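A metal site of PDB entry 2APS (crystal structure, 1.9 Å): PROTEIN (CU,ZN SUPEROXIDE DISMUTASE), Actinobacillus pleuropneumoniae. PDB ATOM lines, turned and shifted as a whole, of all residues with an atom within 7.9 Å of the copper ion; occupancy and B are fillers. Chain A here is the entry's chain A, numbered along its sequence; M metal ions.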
ATOM      1  N   GLY A  53       8.895 -18.189  23.830  1.00  0.00           N
ATOM      2  CA  GLY A  53       8.144 -19.431  23.716  1.00  0.00           C
ATOM      3  C   GLY A  53       9.016 -20.434  22.991  1.00  0.00           C
ATOM      4  O   GLY A  53       9.576 -20.113  21.954  1.00  0.00           O
ATOM      5  N   PHE A  54       9.099 -21.650  23.510  1.00  0.00           N
ATOM      6  CA  PHE A  54       9.944 -22.694  22.949  1.00  0.00           C
ATOM      7  C   PHE A  54       9.071 -23.929  22.784  1.00  0.00           C
ATOM      8  O   PHE A  54       8.597 -24.492  23.781  1.00  0.00           O
ATOM      9  CB  PHE A  54      11.088 -22.958  23.956  1.00  0.00           C
ATOM     10  CG  PHE A  54      12.249 -23.753  23.420  1.00  0.00           C
ATOM     11  CD1 PHE A  54      12.732 -23.557  22.132  1.00  0.00           C
ATOM     12  CD2 PHE A  54      12.910 -24.675  24.241  1.00  0.00           C
ATOM     13  CE1 PHE A  54      13.860 -24.251  21.672  1.00  0.00           C
ATOM     14  CE2 PHE A  54      14.024 -25.367  23.796  1.00  0.00           C
ATOM     15  CZ  PHE A  54      14.506 -25.161  22.506  1.00  0.00           C
ATOM     16  N   HIS A  55       8.775 -24.322  21.546  1.00  0.00           N
ATOM     17  CA  HIS A  55       7.923 -25.493  21.304  1.00  0.00           C
ATOM     18  C   HIS A  55       8.330 -26.275  20.065  1.00  0.00           C
ATOM     19  O   HIS A  55       8.987 -25.753  19.172  1.00  0.00           O
ATOM     20  CB  HIS A  55       6.454 -25.088  21.085  1.00  0.00           C
ATOM     21  CG  HIS A  55       6.038 -23.836  21.789  1.00  0.00           C
ATOM     22  ND1 HIS A  55       5.916 -22.629  21.134  1.00  0.00           N
ATOM     23  CD2 HIS A  55       5.652 -23.612  23.066  1.00  0.00           C
ATOM     24  CE1 HIS A  55       5.458 -21.718  21.973  1.00  0.00           C
ATOM     25  NE2 HIS A  55       5.297 -22.291  23.152  1.00  0.00           N
ATOM     26  N   ILE A  56       7.901 -27.526  20.015  1.00  0.00           N
ATOM     27  CA  ILE A  56       8.175 -28.397  18.875  1.00  0.00           C
ATOM     28  C   ILE A  56       6.901 -28.319  18.029  1.00  0.00           C
ATOM     29  O   ILE A  56       5.798 -28.327  18.573  1.00  0.00           O
ATOM     30  CB  ILE A  56       8.416 -29.864  19.298  1.00  0.00           C
ATOM     31  CG1 ILE A  56       9.713 -29.978  20.116  1.00  0.00           C
ATOM     32  CG2 ILE A  56       8.500 -30.788  18.093  1.00  0.00           C
ATOM     33  CD1 ILE A  56       9.952 -31.370  20.665  1.00  0.00           C
ATOM     34  N   HIS A  57       7.053 -28.165  16.721  1.00  0.00           N
ATOM     35  CA  HIS A  57       5.913 -28.100  15.826  1.00  0.00           C
ATOM     36  C   HIS A  57       5.771 -29.355  14.968  1.00  0.00           C
ATOM     37  O   HIS A  57       6.667 -30.195  14.931  1.00  0.00           O
ATOM     38  CB  HIS A  57       5.985 -26.840  14.956  1.00  0.00           C
ATOM     39  CG  HIS A  57       5.649 -25.583  15.695  1.00  0.00           C
ATOM     40  ND1 HIS A  57       4.639 -24.740  15.309  1.00  0.00           N
ATOM     41  CD2 HIS A  57       6.191 -25.037  16.809  1.00  0.00           C
ATOM     42  CE1 HIS A  57       4.557 -23.722  16.159  1.00  0.00           C
ATOM     43  NE2 HIS A  57       5.499 -23.881  17.074  1.00  0.00           N
ATOM     44  N   ALA A  77       6.009 -25.233   9.415  1.00  0.00           N
ATOM     45  CA  ALA A  77       6.089 -26.099  10.588  1.00  0.00           C
ATOM     46  C   ALA A  77       4.693 -26.520  11.032  1.00  0.00           C
ATOM     47  O   ALA A  77       4.499 -27.605  11.579  1.00  0.00           O
ATOM     48  CB  ALA A  77       6.803 -25.371  11.709  1.00  0.00           C
ATOM     49  N   GLY A  78       3.721 -25.649  10.777  1.00  0.00           N
ATOM     50  CA  GLY A  78       2.342 -25.930  11.155  1.00  0.00           C
ATOM     51  C   GLY A  78       2.053 -25.515  12.578  1.00  0.00           C
ATOM     52  O   GLY A  78       2.571 -24.512  13.073  1.00  0.00           O
ATOM     53  N   GLY A  79       1.187 -26.278  13.253  1.00  0.00           N
ATOM     54  CA  GLY A  79       0.855 -25.983  14.628  1.00  0.00           C
ATOM     55  C   GLY A  79       1.824 -26.696  15.558  1.00  0.00           C
ATOM     56  O   GLY A  79       2.803 -27.294  15.118  1.00  0.00           O
ATOM     57  N   HIS A  80       1.548 -26.624  16.859  1.00  0.00           N
ATOM     58  CA  HIS A  80       2.387 -27.280  17.849  1.00  0.00           C
ATOM     59  C   HIS A  80       2.248 -28.782  17.664  1.00  0.00           C
ATOM     60  O   HIS A  80       1.191 -29.261  17.235  1.00  0.00           O
ATOM     61  CB  HIS A  80       1.970 -26.864  19.273  1.00  0.00           C
ATOM     62  CG  HIS A  80       2.268 -25.432  19.614  1.00  0.00           C
ATOM     63  ND1 HIS A  80       2.138 -24.928  20.894  1.00  0.00           N
ATOM     64  CD2 HIS A  80       2.708 -24.405  18.852  1.00  0.00           C
ATOM     65  CE1 HIS A  80       2.470 -23.648  20.886  1.00  0.00           C
ATOM     66  NE2 HIS A  80       2.818 -23.310  19.665  1.00  0.00           N
ATOM     67  N   TRP A  81       3.305 -29.537  17.939  1.00  0.00           N
ATOM     68  CA  TRP A  81       3.271 -30.982  17.818  1.00  0.00           C
ATOM     69  C   TRP A  81       2.344 -31.505  18.913  1.00  0.00           C
ATOM     70  O   TRP A  81       2.576 -31.245  20.099  1.00  0.00           O
ATOM     71  CB  TRP A  81       4.685 -31.547  17.957  1.00  0.00           C
ATOM     72  CG  TRP A  81       4.790 -33.028  17.895  1.00  0.00           C
ATOM     73  CD1 TRP A  81       4.094 -33.870  17.082  1.00  0.00           C
ATOM     74  CD2 TRP A  81       5.627 -33.847  18.702  1.00  0.00           C
ATOM     75  NE1 TRP A  81       4.438 -35.176  17.336  1.00  0.00           N
ATOM     76  CE2 TRP A  81       5.386 -35.189  18.330  1.00  0.00           C
ATOM     77  CE3 TRP A  81       6.570 -33.587  19.711  1.00  0.00           C
ATOM     78  CZ2 TRP A  81       6.051 -36.264  18.928  1.00  0.00           C
ATOM     79  CZ3 TRP A  81       7.227 -34.654  20.300  1.00  0.00           C
ATOM     80  CH2 TRP A  81       6.956 -35.983  19.910  1.00  0.00           C
ATOM     81  N   HIS A  89      -2.836 -25.985  24.854  1.00  0.00           N
ATOM     82  CA  HIS A  89      -1.470 -25.608  25.153  1.00  0.00           C
ATOM     83  C   HIS A  89      -1.354 -25.559  26.675  1.00  0.00           C
ATOM     84  O   HIS A  89      -2.286 -25.115  27.345  1.00  0.00           O
ATOM     85  CB  HIS A  89      -1.177 -24.235  24.565  1.00  0.00           C
ATOM     86  CG  HIS A  89       0.230 -23.789  24.765  1.00  0.00           C
ATOM     87  ND1 HIS A  89       1.277 -24.354  24.074  1.00  0.00           N
ATOM     88  CD2 HIS A  89       0.763 -22.854  25.585  1.00  0.00           C
ATOM     89  CE1 HIS A  89       2.411 -23.785  24.464  1.00  0.00           C
ATOM     90  NE2 HIS A  89       2.120 -22.881  25.384  1.00  0.00           N
ATOM     91  N   GLY A 100       4.665 -31.225  22.437  1.00  0.00           N
ATOM     92  CA  GLY A 100       5.751 -30.360  22.003  1.00  0.00           C
ATOM     93  C   GLY A 100       5.978 -29.106  22.831  1.00  0.00           C
ATOM     94  O   GLY A 100       6.813 -28.264  22.464  1.00  0.00           O
ATOM     95  N   ASP A 101       5.242 -28.941  23.916  1.00  0.00           N
ATOM     96  CA  ASP A 101       5.377 -27.767  24.781  1.00  0.00           C
ATOM     97  C   ASP A 101       6.585 -27.884  25.696  1.00  0.00           C
ATOM     98  O   ASP A 101       6.567 -28.672  26.644  1.00  0.00           O
ATOM     99  CB  ASP A 101       4.105 -27.557  25.612  1.00  0.00           C
ATOM    100  CG  ASP A 101       2.909 -27.193  24.763  1.00  0.00           C
ATOM    101  OD1 ASP A 101       3.086 -26.841  23.570  1.00  0.00           O
ATOM    102  OD2 ASP A 101       1.767 -27.250  25.290  1.00  0.00           O
ATOM    103  N   SER A 132       9.610 -29.811  13.795  1.00  0.00           N
ATOM    104  CA  SER A 132      10.420 -28.594  13.915  1.00  0.00           C
ATOM    105  C   SER A 132      10.586 -28.098  15.347  1.00  0.00           C
ATOM    106  O   SER A 132       9.858 -28.510  16.249  1.00  0.00           O
ATOM    107  CB  SER A 132       9.829 -27.482  13.042  1.00  0.00           C
ATOM    108  OG  SER A 132       8.406 -27.506  13.074  1.00  0.00           O
ATOM    109  N   LEU A 133      11.540 -27.185  15.524  1.00  0.00           N
ATOM    110  CA  LEU A 133      11.824 -26.599  16.828  1.00  0.00           C
ATOM    111  C   LEU A 133      11.610 -25.114  16.626  1.00  0.00           C
ATOM    112  O   LEU A 133      12.349 -24.488  15.865  1.00  0.00           O
ATOM    113  CB  LEU A 133      13.263 -26.907  17.227  1.00  0.00           C
ATOM    114  CG  LEU A 133      13.679 -26.704  18.690  1.00  0.00           C
ATOM    115  CD1 LEU A 133      12.758 -27.489  19.613  1.00  0.00           C
ATOM    116  CD2 LEU A 133      15.114 -27.156  18.857  1.00  0.00           C
ATOM    117  N   MET A 134      10.612 -24.554  17.281  1.00  0.00           N
ATOM    118  CA  MET A 134      10.299 -23.138  17.121  1.00  0.00           C
ATOM    119  C   MET A 134      10.631 -22.285  18.325  1.00  0.00           C
ATOM    120  O   MET A 134      10.435 -22.703  19.470  1.00  0.00           O
ATOM    121  CB  MET A 134       8.811 -22.993  16.832  1.00  0.00           C
ATOM    122  CG  MET A 134       8.404 -21.640  16.266  1.00  0.00           C
ATOM    123  SD  MET A 134       8.966 -21.454  14.562  1.00  0.00           S
ATOM    124  CE  MET A 134       8.097 -22.822  13.774  1.00  0.00           C
ATOM    125  N   ILE A 135      11.087 -21.064  18.053  1.00  0.00           N
ATOM    126  CA  ILE A 135      11.426 -20.090  19.085  1.00  0.00           C
ATOM    127  C   ILE A 135      10.663 -18.826  18.723  1.00  0.00           C
ATOM    128  O   ILE A 135      10.966 -18.173  17.726  1.00  0.00           O
ATOM    129  CB  ILE A 135      12.944 -19.781  19.122  1.00  0.00           C
ATOM    130  CG1 ILE A 135      13.747 -21.057  19.385  1.00  0.00           C
ATOM    131  CG2 ILE A 135      13.244 -18.744  20.204  1.00  0.00           C
ATOM    132  CD1 ILE A 135      15.235 -20.861  19.357  1.00  0.00           C
ATOM    133  N   HIS A 136       9.656 -18.478  19.521  1.00  0.00           N
ATOM    134  CA  HIS A 136       8.839 -17.305  19.265  1.00  0.00           C
ATOM    135  C   HIS A 136       9.435 -16.003  19.767  1.00  0.00           C
ATOM    136  O   HIS A 136      10.428 -15.968  20.498  1.00  0.00           O
ATOM    137  CB  HIS A 136       7.438 -17.470  19.854  1.00  0.00           C
ATOM    138  CG  HIS A 136       6.722 -18.686  19.359  1.00  0.00           C
ATOM    139  ND1 HIS A 136       5.613 -18.620  18.536  1.00  0.00           N
ATOM    140  CD2 HIS A 136       6.952 -20.004  19.560  1.00  0.00           C
ATOM    141  CE1 HIS A 136       5.196 -19.845  18.267  1.00  0.00           C
ATOM    142  NE2 HIS A 136       5.988 -20.708  18.881  1.00  0.00           N
ATOM    143  N   ASP A 140       5.620 -17.165  27.055  1.00  0.00           N
ATOM    144  CA  ASP A 140       4.748 -18.325  27.133  1.00  0.00           C
ATOM    145  C   ASP A 140       4.228 -18.438  28.552  1.00  0.00           C
ATOM    146  O   ASP A 140       4.993 -18.701  29.483  1.00  0.00           O
ATOM    147  CB  ASP A 140       5.580 -19.572  26.794  1.00  0.00           C
ATOM    148  CG  ASP A 140       4.732 -20.817  26.543  1.00  0.00           C
ATOM    149  OD1 ASP A 140       3.531 -20.826  26.876  1.00  0.00           O
ATOM    150  OD2 ASP A 140       5.274 -21.789  25.997  1.00  0.00           O
ATOM    151  N   LEU A 149      -2.098 -20.400  22.439  1.00  0.00           N
ATOM    152  CA  LEU A 149      -0.751 -20.975  22.443  1.00  0.00           C
ATOM    153  C   LEU A 149       0.289 -20.254  23.321  1.00  0.00           C
ATOM    154  O   LEU A 149       1.433 -20.072  22.913  1.00  0.00           O
ATOM    155  CB  LEU A 149      -0.212 -21.125  21.005  1.00  0.00           C
ATOM    156  CG  LEU A 149      -0.836 -22.082  19.972  1.00  0.00           C
ATOM    157  CD1 LEU A 149      -1.268 -23.380  20.608  1.00  0.00           C
ATOM    158  CD2 LEU A 149      -2.012 -21.434  19.289  1.00  0.00           C
ATOM    159  N   GLY A 152       3.016 -16.577  22.425  1.00  0.00           N
ATOM    160  CA  GLY A 152       4.317 -16.403  21.821  1.00  0.00           C
ATOM    161  C   GLY A 152       4.247 -15.482  20.619  1.00  0.00           C
ATOM    162  O   GLY A 152       5.131 -14.654  20.417  1.00  0.00           O
ATOM    163  N   GLY A 153       3.204 -15.633  19.816  1.00  0.00           N
ATOM    164  CA  GLY A 153       3.013 -14.794  18.652  1.00  0.00           C
ATOM    165  C   GLY A 153       3.887 -15.154  17.456  1.00  0.00           C
ATOM    166  O   GLY A 153       4.004 -16.336  17.110  1.00  0.00           O
ATOM    167  N   PRO A 154       4.503 -14.143  16.814  1.00  0.00           N
ATOM    168  CA  PRO A 154       5.379 -14.330  15.644  1.00  0.00           C
ATOM    169  C   PRO A 154       6.542 -15.284  15.919  1.00  0.00           C
ATOM    170  O   PRO A 154       7.163 -15.250  16.992  1.00  0.00           O
ATOM    171  CB  PRO A 154       5.855 -12.908  15.341  1.00  0.00           C
ATOM    172  CG  PRO A 154       5.726 -12.198  16.654  1.00  0.00           C
ATOM    173  CD  PRO A 154       4.426 -12.723  17.184  1.00  0.00           C
ATOM    174  N   ARG A 155       6.839 -16.105  14.919  1.00  0.00           N
ATOM    175  CA  ARG A 155       7.913 -17.097  15.000  1.00  0.00           C
ATOM    176  C   ARG A 155       9.278 -16.495  14.661  1.00  0.00           C
ATOM    177  O   ARG A 155       9.634 -16.361  13.487  1.00  0.00           O
ATOM    178  CB  ARG A 155       7.564 -18.271  14.080  1.00  0.00           C
ATOM    179  CG  ARG A 155       6.119 -18.702  14.264  1.00  0.00           C
ATOM    180  CD  ARG A 155       5.739 -19.897  13.431  1.00  0.00           C
ATOM    181  NE  ARG A 155       4.331 -20.240  13.664  1.00  0.00           N
ATOM    182  CZ  ARG A 155       3.790 -21.418  13.377  1.00  0.00           C
ATOM    183  NH1 ARG A 155       4.523 -22.384  12.834  1.00  0.00           N
ATOM    184  NH2 ARG A 155       2.517 -21.636  13.649  1.00  0.00           N
ATOM    185  N   ALA A 157      12.553 -17.692  15.448  1.00  0.00           N
ATOM    186  CA  ALA A 157      13.619 -18.603  15.010  1.00  0.00           C
ATOM    187  C   ALA A 157      13.079 -20.027  14.854  1.00  0.00           C
ATOM    188  O   ALA A 157      12.075 -20.377  15.487  1.00  0.00           O
ATOM    189  CB  ALA A 157      14.784 -18.583  15.985  1.00  0.00           C
HETATM  190 CU    CU M   1       5.545 -22.542  18.869  1.00  0.00          CU
HETATM  191 ZN    ZN M   2       1.550 -25.901  22.689  1.00  0.00          ZN
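O of His 55 lies within hydrogen-bond range of N of Met 134, 2.8 Å away.
A ring nitrogen (ND1) of His 57 sits at hydrogen-bond distance from the backbone carbonyl oxygen of Gly 78, 3.1 Å away.
The backbone NH (N) of His 57 lies within hydrogen-bond range of the backbone carbonyl oxygen (O) of Ser 132 (2.9 Å).
The side-chain carboxylate (OD2) of Asp 140 sits at hydrogen-bond distance from a ring nitrogen (NE2) of His 55 (2.9 Å).
A ring nitrogen (ND1) of His 136 is in hydrogen-bond range of the backbone carbonyl oxygen (O) of Gly 153 (3.1 Å).
ND1 of His 57 sits at hydrogen-bond distance from NH1 of Arg 155, 3.4 Å away.
A ring nitrogen (ND1) of His 55 sits close to a ring nitrogen (NE2) of His 80, at 3.5 Å.
The backbone carbonyl oxygen (O) of Gly 53 sits at hydrogen-bond distance from the backbone NH (N) of His 136, 2.9 Å away.
Merely in contact with the copper ion: His 80 (2.9 Å) and Met 134 (3.9 Å).
Within 4 Å of the copper ion: His 55, His 57, His 80, Met 134 and His 136.
The nearest printed residue that does not touch the copper ion is Phe 54 (5.4 Å).
The copper ion is bound by NE2 of His 136 (1.9 Å), NE2 of His 57 (2.2 Å) and ND1 of His 55 (2.3 Å).
The copper ion has three donor atoms within binding distance.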
